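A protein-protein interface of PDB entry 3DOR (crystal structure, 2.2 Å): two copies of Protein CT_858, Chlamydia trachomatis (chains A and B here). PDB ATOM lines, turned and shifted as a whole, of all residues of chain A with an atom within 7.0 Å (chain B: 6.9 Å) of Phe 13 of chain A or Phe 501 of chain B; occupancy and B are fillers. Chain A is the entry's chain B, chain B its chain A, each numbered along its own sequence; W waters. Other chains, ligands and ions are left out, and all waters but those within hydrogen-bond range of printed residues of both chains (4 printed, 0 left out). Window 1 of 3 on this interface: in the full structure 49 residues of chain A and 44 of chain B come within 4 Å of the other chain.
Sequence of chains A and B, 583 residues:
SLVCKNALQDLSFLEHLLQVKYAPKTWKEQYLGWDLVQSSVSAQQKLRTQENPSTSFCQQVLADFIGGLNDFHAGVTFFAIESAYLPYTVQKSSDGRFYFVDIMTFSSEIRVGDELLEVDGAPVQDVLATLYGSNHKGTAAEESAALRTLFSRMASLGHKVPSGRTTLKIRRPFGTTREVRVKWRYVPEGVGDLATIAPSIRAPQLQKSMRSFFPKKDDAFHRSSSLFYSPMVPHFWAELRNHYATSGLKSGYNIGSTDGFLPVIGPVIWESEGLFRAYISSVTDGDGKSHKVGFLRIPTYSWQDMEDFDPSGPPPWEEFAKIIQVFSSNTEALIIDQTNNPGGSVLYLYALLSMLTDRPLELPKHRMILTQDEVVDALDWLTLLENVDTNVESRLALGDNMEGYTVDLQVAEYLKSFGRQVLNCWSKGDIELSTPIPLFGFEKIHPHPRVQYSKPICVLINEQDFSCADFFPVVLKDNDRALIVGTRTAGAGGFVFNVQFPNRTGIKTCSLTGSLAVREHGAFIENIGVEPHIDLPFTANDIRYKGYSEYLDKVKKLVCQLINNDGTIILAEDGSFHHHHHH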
ATOM      1  N   ALA A   7       2.849 -16.394  31.045  1.00  0.00           N
ATOM      2  CA  ALA A   7       4.154 -16.895  30.640  1.00  0.00           C
ATOM      3  C   ALA A   7       3.980 -18.227  29.932  1.00  0.00           C
ATOM      4  O   ALA A   7       4.587 -18.473  28.894  1.00  0.00           O
ATOM      5  CB  ALA A   7       5.058 -17.058  31.858  1.00  0.00           C
ATOM      6  N   LEU A   8       3.144 -19.090  30.499  1.00  0.00           N
ATOM      7  CA  LEU A   8       2.891 -20.394  29.904  1.00  0.00           C
ATOM      8  C   LEU A   8       2.212 -20.220  28.552  1.00  0.00           C
ATOM      9  O   LEU A   8       2.521 -20.931  27.588  1.00  0.00           O
ATOM     10  CB  LEU A   8       1.997 -21.232  30.824  1.00  0.00           C
ATOM     11  CG  LEU A   8       2.639 -21.882  32.057  1.00  0.00           C
ATOM     12  CD1 LEU A   8       1.551 -22.297  33.051  1.00  0.00           C
ATOM     13  CD2 LEU A   8       3.459 -23.093  31.626  1.00  0.00           C
ATOM     14  N   GLN A   9       1.279 -19.273  28.488  1.00  0.00           N
ATOM     15  CA  GLN A   9       0.551 -19.010  27.253  1.00  0.00           C
ATOM     16  C   GLN A   9       1.517 -18.566  26.156  1.00  0.00           C
ATOM     17  O   GLN A   9       1.529 -19.114  25.055  1.00  0.00           O
ATOM     18  CB  GLN A   9      -0.487 -17.909  27.478  1.00  0.00           C
ATOM     19  CG  GLN A   9      -1.846 -18.200  26.875  1.00  0.00           C
ATOM     20  CD  GLN A   9      -1.772 -18.570  25.408  1.00  0.00           C
ATOM     21  OE1 GLN A   9      -1.309 -17.785  24.580  1.00  0.00           O
ATOM     22  NE2 GLN A   9      -2.229 -19.775  25.079  1.00  0.00           N
ATOM     23  N   ASP A  10       2.338 -17.570  26.463  1.00  0.00           N
ATOM     24  CA  ASP A  10       3.277 -17.062  25.479  1.00  0.00           C
ATOM     25  C   ASP A  10       4.343 -18.092  25.111  1.00  0.00           C
ATOM     26  O   ASP A  10       4.793 -18.145  23.964  1.00  0.00           O
ATOM     27  CB  ASP A  10       3.896 -15.751  25.981  1.00  0.00           C
ATOM     28  CG  ASP A  10       2.852 -14.655  26.151  1.00  0.00           C
ATOM     29  OD1 ASP A  10       1.979 -14.529  25.264  1.00  0.00           O
ATOM     30  OD2 ASP A  10       2.897 -13.918  27.158  1.00  0.00           O
ATOM     31  N   LEU A  11       4.724 -18.924  26.075  1.00  0.00           N
ATOM     32  CA  LEU A  11       5.711 -19.966  25.820  1.00  0.00           C
ATOM     33  C   LEU A  11       5.095 -20.899  24.786  1.00  0.00           C
ATOM     34  O   LEU A  11       5.732 -21.265  23.797  1.00  0.00           O
ATOM     35  CB  LEU A  11       6.004 -20.761  27.100  1.00  0.00           C
ATOM     36  CG  LEU A  11       7.315 -21.551  27.226  1.00  0.00           C
ATOM     37  CD1 LEU A  11       7.183 -22.532  28.378  1.00  0.00           C
ATOM     38  CD2 LEU A  11       7.642 -22.301  25.957  1.00  0.00           C
ATOM     39  N   SER A  12       3.840 -21.272  25.015  1.00  0.00           N
ATOM     40  CA  SER A  12       3.156 -22.176  24.102  1.00  0.00           C
ATOM     41  C   SER A  12       3.082 -21.571  22.711  1.00  0.00           C
ATOM     42  O   SER A  12       3.141 -22.284  21.711  1.00  0.00           O
ATOM     43  CB  SER A  12       1.742 -22.497  24.604  1.00  0.00           C
ATOM     44  OG  SER A  12       0.873 -21.389  24.437  1.00  0.00           O
ATOM     45  N   PHE A  13       2.939 -20.251  22.639  1.00  0.00           N
ATOM     46  CA  PHE A  13       2.887 -19.606  21.336  1.00  0.00           C
ATOM     47  C   PHE A  13       4.253 -19.716  20.657  1.00  0.00           C
ATOM     48  O   PHE A  13       4.343 -20.062  19.476  1.00  0.00           O
ATOM     49  CB  PHE A  13       2.494 -18.133  21.466  1.00  0.00           C
ATOM     50  CG  PHE A  13       2.392 -17.425  20.141  1.00  0.00           C
ATOM     51  CD1 PHE A  13       1.499 -17.872  19.168  1.00  0.00           C
ATOM     52  CD2 PHE A  13       3.195 -16.324  19.862  1.00  0.00           C
ATOM     53  CE1 PHE A  13       1.405 -17.233  17.930  1.00  0.00           C
ATOM     54  CE2 PHE A  13       3.112 -15.672  18.628  1.00  0.00           C
ATOM     55  CZ  PHE A  13       2.214 -16.126  17.659  1.00  0.00           C
ATOM     56  N   LEU A  14       5.317 -19.429  21.404  1.00  0.00           N
ATOM     57  CA  LEU A  14       6.664 -19.519  20.848  1.00  0.00           C
ATOM     58  C   LEU A  14       6.939 -20.931  20.368  1.00  0.00           C
ATOM     59  O   LEU A  14       7.450 -21.134  19.273  1.00  0.00           O
ATOM     60  CB  LEU A  14       7.708 -19.133  21.888  1.00  0.00           C
ATOM     61  CG  LEU A  14       7.692 -17.700  22.400  1.00  0.00           C
ATOM     62  CD1 LEU A  14       8.862 -17.537  23.362  1.00  0.00           C
ATOM     63  CD2 LEU A  14       7.792 -16.707  21.237  1.00  0.00           C
ATOM     64  N   GLU A  15       6.598 -21.911  21.197  1.00  0.00           N
ATOM     65  CA  GLU A  15       6.802 -23.307  20.840  1.00  0.00           C
ATOM     66  C   GLU A  15       6.112 -23.617  19.518  1.00  0.00           C
ATOM     67  O   GLU A  15       6.642 -24.356  18.688  1.00  0.00           O
ATOM     68  CB  GLU A  15       6.246 -24.230  21.931  1.00  0.00           C
ATOM     69  CG  GLU A  15       6.402 -25.710  21.599  1.00  0.00           C
ATOM     70  CD  GLU A  15       5.693 -26.625  22.588  1.00  0.00           C
ATOM     71  OE1 GLU A  15       5.681 -27.854  22.356  1.00  0.00           O
ATOM     72  OE2 GLU A  15       5.152 -26.116  23.595  1.00  0.00           O
ATOM     73  N   HIS A  16       4.923 -23.059  19.316  1.00  0.00           N
ATOM     74  CA  HIS A  16       4.207 -23.322  18.077  1.00  0.00           C
ATOM     75  C   HIS A  16       4.912 -22.668  16.891  1.00  0.00           C
ATOM     76  O   HIS A  16       4.911 -23.208  15.789  1.00  0.00           O
ATOM     77  CB  HIS A  16       2.754 -22.839  18.175  1.00  0.00           C
ATOM     78  CG  HIS A  16       1.977 -23.041  16.914  1.00  0.00           C
ATOM     79  ND1 HIS A  16       1.636 -21.998  16.078  1.00  0.00           N
ATOM     80  CD2 HIS A  16       1.556 -24.172  16.300  1.00  0.00           C
ATOM     81  CE1 HIS A  16       1.042 -22.479  15.001  1.00  0.00           C
ATOM     82  NE2 HIS A  16       0.981 -23.795  15.110  1.00  0.00           N
ATOM     83  N   LEU A  17       5.522 -21.510  17.111  1.00  0.00           N
ATOM     84  CA  LEU A  17       6.242 -20.838  16.029  1.00  0.00           C
ATOM     85  C   LEU A  17       7.424 -21.716  15.603  1.00  0.00           C
ATOM     86  O   LEU A  17       7.771 -21.790  14.424  1.00  0.00           O
ATOM     87  CB  LEU A  17       6.756 -19.465  16.486  1.00  0.00           C
ATOM     88  CG  LEU A  17       5.719 -18.414  16.898  1.00  0.00           C
ATOM     89  CD1 LEU A  17       6.414 -17.097  17.225  1.00  0.00           C
ATOM     90  CD2 LEU A  17       4.714 -18.219  15.779  1.00  0.00           C
ATOM     91  N   LEU A  18       8.025 -22.398  16.576  1.00  0.00           N
ATOM     92  CA  LEU A  18       9.164 -23.270  16.308  1.00  0.00           C
ATOM     93  C   LEU A  18       8.842 -24.480  15.437  1.00  0.00           C
ATOM     94  O   LEU A  18       9.746 -25.102  14.877  1.00  0.00           O
ATOM     95  CB  LEU A  18       9.787 -23.732  17.626  1.00  0.00           C
ATOM     96  CG  LEU A  18      10.331 -22.583  18.475  1.00  0.00           C
ATOM     97  CD1 LEU A  18      11.011 -23.138  19.709  1.00  0.00           C
ATOM     98  CD2 LEU A  18      11.308 -21.755  17.651  1.00  0.00           C
ATOM     99  N   LYS A  21       7.477 -22.149  11.650  1.00  0.00           N
ATOM    100  CA  LYS A  21       8.377 -21.262  10.923  1.00  0.00           C
ATOM    101  C   LYS A  21       9.836 -21.229  11.386  1.00  0.00           C
ATOM    102  O   LYS A  21      10.470 -20.177  11.342  1.00  0.00           O
ATOM    103  CB  LYS A  21       7.827 -19.834  10.956  1.00  0.00           C
ATOM    104  CG  LYS A  21       7.026 -19.440   9.746  1.00  0.00           C
ATOM    105  CD  LYS A  21       7.874 -19.459   8.491  1.00  0.00           C
ATOM    106  CE  LYS A  21       7.471 -18.339   7.544  1.00  0.00           C
ATOM    107  NZ  LYS A  21       7.888 -16.988   8.067  1.00  0.00           N
ATOM    108  N   THR A 371       4.832 -21.200   4.465  1.00  0.00           N
ATOM    109  CA  THR A 371       3.465 -20.949   4.933  1.00  0.00           C
ATOM    110  C   THR A 371       2.827 -20.189   3.765  1.00  0.00           C
ATOM    111  O   THR A 371       3.525 -19.754   2.847  1.00  0.00           O
ATOM    112  CB  THR A 371       3.392 -20.062   6.220  1.00  0.00           C
ATOM    113  OG1 THR A 371       3.889 -18.751   5.939  1.00  0.00           O
ATOM    114  CG2 THR A 371       4.199 -20.680   7.352  1.00  0.00           C
ATOM    115  N   ASP A 373       2.140 -17.333   3.522  1.00  0.00           N
ATOM    116  CA  ASP A 373       2.695 -15.987   3.425  1.00  0.00           C
ATOM    117  C   ASP A 373       3.746 -16.032   2.316  1.00  0.00           C
ATOM    118  O   ASP A 373       3.774 -15.146   1.454  1.00  0.00           O
ATOM    119  CB  ASP A 373       3.338 -15.627   4.746  1.00  0.00           C
ATOM    120  CG  ASP A 373       3.923 -14.200   4.765  1.00  0.00           C
ATOM    121  OD1 ASP A 373       4.315 -13.741   5.856  1.00  0.00           O
ATOM    122  OD2 ASP A 373       3.999 -13.501   3.722  1.00  0.00           O
ATOM    123  N   VAL A 499       8.984 -11.450  14.862  1.00  0.00           N
ATOM    124  CA  VAL A 499       7.592 -11.634  15.209  1.00  0.00           C
ATOM    125  C   VAL A 499       7.256 -10.757  16.402  1.00  0.00           C
ATOM    126  O   VAL A 499       8.027 -10.672  17.351  1.00  0.00           O
ATOM    127  CB  VAL A 499       7.298 -13.111  15.559  1.00  0.00           C
ATOM    128  CG1 VAL A 499       5.832 -13.278  15.922  1.00  0.00           C
ATOM    129  CG2 VAL A 499       7.652 -14.000  14.367  1.00  0.00           C
ATOM    130  N   GLN A 500       6.112 -10.084  16.331  1.00  0.00           N
ATOM    131  CA  GLN A 500       5.643  -9.234  17.411  1.00  0.00           C
ATOM    132  C   GLN A 500       4.202  -9.641  17.671  1.00  0.00           C
ATOM    133  O   GLN A 500       3.522 -10.134  16.777  1.00  0.00           O
ATOM    134  CB  GLN A 500       5.691  -7.754  17.007  1.00  0.00           C
ATOM    135  CG  GLN A 500       7.032  -7.276  16.436  1.00  0.00           C
ATOM    136  CD  GLN A 500       6.967  -6.969  14.936  1.00  0.00           C
ATOM    137  OE1 GLN A 500       7.756  -6.176  14.418  1.00  0.00           O
ATOM    138  NE2 GLN A 500       6.032  -7.600  14.237  1.00  0.00           N
ATOM    139  N   PHE A 501       3.736  -9.453  18.895  1.00  0.00           N
ATOM    140  CA  PHE A 501       2.361  -9.800  19.230  1.00  0.00           C
ATOM    141  C   PHE A 501       2.083  -9.278  20.627  1.00  0.00           C
ATOM    142  O   PHE A 501       2.956  -9.308  21.477  1.00  0.00           O
ATOM    143  CB  PHE A 501       2.158 -11.322  19.158  1.00  0.00           C
ATOM    144  CG  PHE A 501       2.974 -12.098  20.155  1.00  0.00           C
ATOM    145  CD1 PHE A 501       2.426 -12.478  21.378  1.00  0.00           C
ATOM    146  CD2 PHE A 501       4.296 -12.432  19.883  1.00  0.00           C
ATOM    147  CE1 PHE A 501       3.182 -13.178  22.312  1.00  0.00           C
ATOM    148  CE2 PHE A 501       5.060 -13.130  20.813  1.00  0.00           C
ATOM    149  CZ  PHE A 501       4.502 -13.502  22.028  1.00  0.00           C
ATOM    150  N   GLN B   9      -5.088 -24.217  16.927  1.00  0.00           N
ATOM    151  CA  GLN B   9      -3.949 -23.501  17.502  1.00  0.00           C
ATOM    152  C   GLN B   9      -4.128 -21.991  17.279  1.00  0.00           C
ATOM    153  O   GLN B   9      -4.087 -21.199  18.218  1.00  0.00           O
ATOM    154  CB  GLN B   9      -2.643 -23.952  16.840  1.00  0.00           C
ATOM    155  CG  GLN B   9      -1.468 -24.128  17.793  1.00  0.00           C
ATOM    156  CD  GLN B   9      -1.204 -22.909  18.652  1.00  0.00           C
ATOM    157  OE1 GLN B   9      -1.063 -21.794  18.150  1.00  0.00           O
ATOM    158  NE2 GLN B   9      -1.128 -23.117  19.956  1.00  0.00           N
ATOM    159  N   ASP B  10      -4.337 -21.599  16.026  1.00  0.00           N
ATOM    160  CA  ASP B  10      -4.500 -20.185  15.721  1.00  0.00           C
ATOM    161  C   ASP B  10      -5.734 -19.581  16.398  1.00  0.00           C
ATOM    162  O   ASP B  10      -5.716 -18.422  16.823  1.00  0.00           O
ATOM    163  CB  ASP B  10      -4.492 -19.985  14.199  1.00  0.00           C
ATOM    164  CG  ASP B  10      -3.163 -20.420  13.574  1.00  0.00           C
ATOM    165  OD1 ASP B  10      -2.132 -20.251  14.254  1.00  0.00           O
ATOM    166  OD2 ASP B  10      -3.136 -20.921  12.428  1.00  0.00           O
ATOM    167  N   LEU B  11      -6.791 -20.377  16.535  1.00  0.00           N
ATOM    168  CA  LEU B  11      -7.999 -19.909  17.206  1.00  0.00           C
ATOM    169  C   LEU B  11      -7.669 -19.592  18.665  1.00  0.00           C
ATOM    170  O   LEU B  11      -8.050 -18.541  19.184  1.00  0.00           O
ATOM    171  CB  LEU B  11      -9.092 -20.982  17.139  1.00  0.00           C
ATOM    172  CG  LEU B  11     -10.454 -20.740  17.818  1.00  0.00           C
ATOM    173  CD1 LEU B  11     -10.337 -20.953  19.315  1.00  0.00           C
ATOM    174  CD2 LEU B  11     -10.959 -19.337  17.498  1.00  0.00           C
ATOM    175  N   PHE B  13      -4.967 -18.709  19.817  1.00  0.00           N
ATOM    176  CA  PHE B  13      -4.122 -17.522  19.883  1.00  0.00           C
ATOM    177  C   PHE B  13      -5.004 -16.282  19.798  1.00  0.00           C
ATOM    178  O   PHE B  13      -4.853 -15.344  20.580  1.00  0.00           O
ATOM    179  CB  PHE B  13      -3.097 -17.508  18.748  1.00  0.00           C
ATOM    180  CG  PHE B  13      -2.207 -16.296  18.755  1.00  0.00           C
ATOM    181  CD1 PHE B  13      -1.305 -16.087  19.795  1.00  0.00           C
ATOM    182  CD2 PHE B  13      -2.283 -15.354  17.732  1.00  0.00           C
ATOM    183  CE1 PHE B  13      -0.490 -14.958  19.818  1.00  0.00           C
ATOM    184  CE2 PHE B  13      -1.472 -14.218  17.742  1.00  0.00           C
ATOM    185  CZ  PHE B  13      -0.575 -14.018  18.784  1.00  0.00           C
ATOM    186  N   LEU B  14      -5.922 -16.269  18.840  1.00  0.00           N
ATOM    187  CA  LEU B  14      -6.832 -15.139  18.703  1.00  0.00           C
ATOM    188  C   LEU B  14      -7.608 -14.965  20.007  1.00  0.00           C
ATOM    189  O   LEU B  14      -7.828 -13.847  20.473  1.00  0.00           O
ATOM    190  CB  LEU B  14      -7.803 -15.373  17.544  1.00  0.00           C
ATOM    191  CG  LEU B  14      -7.164 -15.375  16.152  1.00  0.00           C
ATOM    192  CD1 LEU B  14      -8.234 -15.648  15.096  1.00  0.00           C
ATOM    193  CD2 LEU B  14      -6.483 -14.030  15.901  1.00  0.00           C
ATOM    194  N   LEU B  17      -5.593 -13.135  22.564  1.00  0.00           N
ATOM    195  CA  LEU B  17      -5.460 -11.717  22.236  1.00  0.00           C
ATOM    196  C   LEU B  17      -6.701 -10.960  22.701  1.00  0.00           C
ATOM    197  O   LEU B  17      -6.613  -9.829  23.180  1.00  0.00           O
ATOM    198  CB  LEU B  17      -5.291 -11.520  20.724  1.00  0.00           C
ATOM    199  CG  LEU B  17      -4.034 -12.080  20.050  1.00  0.00           C
ATOM    200  CD1 LEU B  17      -4.050 -11.722  18.577  1.00  0.00           C
ATOM    201  CD2 LEU B  17      -2.788 -11.504  20.713  1.00  0.00           C
ATOM    202  N   PHE B  79      -4.149 -14.785   3.595  1.00  0.00           N
ATOM    203  CA  PHE B  79      -3.299 -14.841   2.413  1.00  0.00           C
ATOM    204  C   PHE B  79      -4.043 -15.746   1.426  1.00  0.00           C
ATOM    205  O   PHE B  79      -3.716 -16.924   1.275  1.00  0.00           O
ATOM    206  CB  PHE B  79      -1.929 -15.464   2.743  1.00  0.00           C
ATOM    207  CG  PHE B  79      -1.038 -14.594   3.602  1.00  0.00           C
ATOM    208  CD1 PHE B  79      -0.715 -14.980   4.908  1.00  0.00           C
ATOM    209  CD2 PHE B  79      -0.495 -13.411   3.097  1.00  0.00           C
ATOM    210  CE1 PHE B  79       0.143 -14.202   5.707  1.00  0.00           C
ATOM    211  CE2 PHE B  79       0.367 -12.622   3.886  1.00  0.00           C
ATOM    212  CZ  PHE B  79       0.685 -13.022   5.196  1.00  0.00           C
ATOM    213  N   VAL B 499      -2.194  -7.171  14.172  1.00  0.00           N
ATOM    214  CA  VAL B 499      -1.317  -8.231  14.632  1.00  0.00           C
ATOM    215  C   VAL B 499      -1.070  -9.202  13.488  1.00  0.00           C
ATOM    216  O   VAL B 499      -2.000  -9.592  12.781  1.00  0.00           O
ATOM    217  CB  VAL B 499      -1.949  -9.014  15.816  1.00  0.00           C
ATOM    218  CG1 VAL B 499      -0.981 -10.087  16.313  1.00  0.00           C
ATOM    219  CG2 VAL B 499      -2.301  -8.060  16.946  1.00  0.00           C
ATOM    220  N   GLN B 500       0.189  -9.568  13.296  1.00  0.00           N
ATOM    221  CA  GLN B 500       0.556 -10.536  12.269  1.00  0.00           C
ATOM    222  C   GLN B 500       1.372 -11.584  12.990  1.00  0.00           C
ATOM    223  O   GLN B 500       1.989 -11.294  14.013  1.00  0.00           O
ATOM    224  CB  GLN B 500       1.441  -9.912  11.192  1.00  0.00           C
ATOM    225  CG  GLN B 500       0.920  -8.647  10.591  1.00  0.00           C
ATOM    226  CD  GLN B 500       1.909  -7.527  10.783  1.00  0.00           C
ATOM    227  OE1 GLN B 500       1.992  -6.933  11.863  1.00  0.00           O
ATOM    228  NE2 GLN B 500       2.696  -7.249   9.741  1.00  0.00           N
ATOM    229  N   PHE B 501       1.385 -12.796  12.464  1.00  0.00           N
ATOM    230  CA  PHE B 501       2.164 -13.852  13.077  1.00  0.00           C
ATOM    231  C   PHE B 501       2.242 -15.019  12.114  1.00  0.00           C
ATOM    232  O   PHE B 501       1.307 -15.270  11.358  1.00  0.00           O
ATOM    233  CB  PHE B 501       1.535 -14.275  14.417  1.00  0.00           C
ATOM    234  CG  PHE B 501       0.128 -14.805  14.300  1.00  0.00           C
ATOM    235  CD1 PHE B 501      -0.116 -16.178  14.292  1.00  0.00           C
ATOM    236  CD2 PHE B 501      -0.954 -13.934  14.209  1.00  0.00           C
ATOM    237  CE1 PHE B 501      -1.421 -16.674  14.197  1.00  0.00           C
ATOM    238  CE2 PHE B 501      -2.266 -14.416  14.112  1.00  0.00           C
ATOM    239  CZ  PHE B 501      -2.499 -15.783  14.106  1.00  0.00           C
ATOM    240  N   PRO B 502       3.385 -15.722  12.088  1.00  0.00           N
ATOM    241  CA  PRO B 502       3.496 -16.862  11.175  1.00  0.00           C
ATOM    242  C   PRO B 502       2.457 -17.898  11.572  1.00  0.00           C
ATOM    243  O   PRO B 502       2.174 -18.055  12.751  1.00  0.00           O
ATOM    244  CB  PRO B 502       4.935 -17.344  11.382  1.00  0.00           C
ATOM    245  CG  PRO B 502       5.282 -16.855  12.767  1.00  0.00           C
ATOM    246  CD  PRO B 502       4.637 -15.498  12.832  1.00  0.00           C
ATOM    247  N   ASN B 503       1.878 -18.584  10.594  1.00  0.00           N
ATOM    248  CA  ASN B 503       0.859 -19.580  10.891  1.00  0.00           C
ATOM    249  C   ASN B 503       0.549 -20.331   9.613  1.00  0.00           C
ATOM    250  O   ASN B 503       0.898 -19.882   8.525  1.00  0.00           O
ATOM    251  CB  ASN B 503      -0.404 -18.886  11.400  1.00  0.00           C
ATOM    252  CG  ASN B 503      -1.115 -18.101  10.304  1.00  0.00           C
ATOM    253  OD1 ASN B 503      -1.964 -18.644   9.588  1.00  0.00           O
ATOM    254  ND2 ASN B 503      -0.753 -16.826  10.153  1.00  0.00           N
ATOM    255  N   ARG B 504      -0.116 -21.473   9.736  1.00  0.00           N
ATOM    256  CA  ARG B 504      -0.451 -22.249   8.552  1.00  0.00           C
ATOM    257  C   ARG B 504      -1.931 -22.244   8.177  1.00  0.00           C
ATOM    258  O   ARG B 504      -2.363 -22.995   7.302  1.00  0.00           O
ATOM    259  CB  ARG B 504       0.094 -23.675   8.700  1.00  0.00           C
ATOM    260  CG  ARG B 504       1.605 -23.660   8.586  1.00  0.00           C
ATOM    261  CD  ARG B 504       2.270 -25.009   8.640  1.00  0.00           C
ATOM    262  NE  ARG B 504       3.612 -24.871   8.083  1.00  0.00           N
ATOM    263  CZ  ARG B 504       4.616 -25.711   8.289  1.00  0.00           C
ATOM    264  NH1 ARG B 504       4.453 -26.783   9.055  1.00  0.00           N
ATOM    265  NH2 ARG B 504       5.788 -25.471   7.720  1.00  0.00           N
ATOM    266  N   ILE B 507      -3.491 -16.911   7.921  1.00  0.00           N
ATOM    267  CA  ILE B 507      -3.925 -15.667   8.515  1.00  0.00           C
ATOM    268  C   ILE B 507      -2.890 -14.577   8.226  1.00  0.00           C
ATOM    269  O   ILE B 507      -1.712 -14.706   8.573  1.00  0.00           O
ATOM    270  CB  ILE B 507      -4.116 -15.828  10.031  1.00  0.00           C
ATOM    271  CG1 ILE B 507      -5.170 -16.912  10.302  1.00  0.00           C
ATOM    272  CG2 ILE B 507      -4.547 -14.504  10.646  1.00  0.00           C
ATOM    273  CD1 ILE B 507      -5.358 -17.221  11.771  1.00  0.00           C
ATOM    274  N   LYS B 508      -3.342 -13.513   7.576  1.00  0.00           N
ATOM    275  CA  LYS B 508      -2.470 -12.409   7.227  1.00  0.00           C
ATOM    276  C   LYS B 508      -2.452 -11.335   8.309  1.00  0.00           C
ATOM    277  O   LYS B 508      -1.386 -10.891   8.730  1.00  0.00           O
ATOM    278  CB  LYS B 508      -2.910 -11.798   5.899  1.00  0.00           C
ATOM    279  CG  LYS B 508      -2.135 -10.545   5.517  1.00  0.00           C
ATOM    280  CD  LYS B 508      -2.497 -10.083   4.121  1.00  0.00           C
ATOM    281  CE  LYS B 508      -1.763  -8.798   3.779  1.00  0.00           C
ATOM    282  NZ  LYS B 508      -1.865  -8.485   2.330  1.00  0.00           N
ATOM    283  N   THR B 509      -3.630 -10.924   8.763  1.00  0.00           N
ATOM    284  CA  THR B 509      -3.714  -9.894   9.789  1.00  0.00           C
ATOM    285  C   THR B 509      -4.991 -10.028  10.602  1.00  0.00           C
ATOM    286  O   THR B 509      -6.007 -10.509  10.109  1.00  0.00           O
ATOM    287  CB  THR B 509      -3.732  -8.465   9.177  1.00  0.00           C
ATOM    288  OG1 THR B 509      -2.620  -8.292   8.298  1.00  0.00           O
ATOM    289  CG2 THR B 509      -3.652  -7.423  10.269  1.00  0.00           C
ATOM    290  N   CYS B 510      -4.920  -9.615  11.861  1.00  0.00           N
ATOM    291  CA  CYS B 510      -6.088  -9.612  12.710  1.00  0.00           C
ATOM    292  C   CYS B 510      -6.066  -8.255  13.371  1.00  0.00           C
ATOM    293  O   CYS B 510      -5.195  -7.972  14.193  1.00  0.00           O
ATOM    294  CB  CYS B 510      -6.044 -10.694  13.778  1.00  0.00           C
ATOM    295  SG  CYS B 510      -7.516 -10.590  14.853  1.00  0.00           S
HETATM  296  O   HOH W   1      -0.646 -22.312  12.437  1.00  0.00           O
HETATM  297  O   HOH W   2       4.778 -10.302  13.833  1.00  0.00           O
HETATM  298  O   HOH W   3       2.096  -8.177  14.990  1.00  0.00           O
HETATM  299  O   HOH W   4       2.592 -17.132   8.192  1.00  0.00           O
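Phe 501 of chain B touches just one residue of chain A: Phe 13.
Of the printed residues of chain A, Asp 10 of chain B touches His 16 (3.9 Å).
Of the printed residues of chain B, Leu 17 of chain A touches Pro 502 (3.4 Å).
Of the printed residues of chain B, His 16 of chain A touches Gln 9 (3.4 Å) and Asp 10 (3.9 Å).
Of the printed residues of chain B, Thr 371 of chain A touches Asn 503 (3.4 Å).
Gln 9 of chain A touches none of the printed residues of chain B.
Water W1 lies within hydrogen-bond range of OD2 of Asp 10 of chain B (2.9 Å), N of Arg 504 of chain B (2.9 Å) and NE2 of His 16 of chain A (3.5 Å).
Water W4 lies within hydrogen-bond range of the backbone NH (N) of Asn 503 of chain B (2.9 Å) and the side-chain hydroxyl (OG1) of Thr 371 of chain A (3.1 Å).
Phe 13 of chain A touches Phe 13 of chain B (CD1 to CD1, 3.4 Å).
Phe 501 of chain B touches Phe 13 of chain A.
His 16 of chain A touches Asp 10 of chain B.
CB of Thr 371 of chain A touches O of Asn 503 of chain B, 3.4 Å away.
Phe 79 of chain B touches Asp 373 of chain A (CZ to CG, 3.5 Å).
Val 499 of chain A touches Pro 502 of chain B.
CB of Phe 501 of chain A touches CZ of Phe 13 of chain B (3.9 Å).
ND2 of Asn 503 of chain B is in hydrogen-bond range of O of Phe 501 of chain B (2.8 Å).
O of Ile 507 of chain B sits at hydrogen-bond distance from ND2 of Asn 503 of chain B (2.8 Å).
The backbone NH (N) of Asp 373 of chain A lies close to the side-chain hydroxyl (OG1) of Thr 371 of chain A (3.3 Å).
The side-chain amide oxygen (OE1) of Gln 9 of chain B lies within hydrogen-bond range of a ring nitrogen (ND1) of His 16 of chain A, 3.4 Å away.
The backbone carbonyl oxygen of Gln 500 of chain B lies close to the backbone carbonyl oxygen of Gln 500 of chain A, 3.4 Å away.
Phe 13 of chain B touches its own counterpart, Phe 13 of chain A.
Gln 500 of chain B touches its own counterpart, Gln 500 of chain A.
Positions printed for both chains: 9, 10, 11, 13, 14, 17, 499, 500 and 501.
Of the 11 pairs that touch across the chains among the printed residues, 4 have their exchanged pair printed and touching as well.
Of the 17 printed residues of chain B, 8 touch a printed residue of chain A.
Printed residues of chain B that touch a printed residue of chain A: Gln 9, Asp 10, Phe 13, Phe 79, Gln 500, Phe 501, Pro 502 and Asn 503.
Hydrophobic or aromatic side chains of chain B within 4 Å of the printed part of chain A: Phe 13, Phe 79, Phe 501 and Pro 502.
Along chain B the printed residues that touch a printed residue of chain A span positions 9 to 503.
Among the printed residues, 11 pairs touch across the chains.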
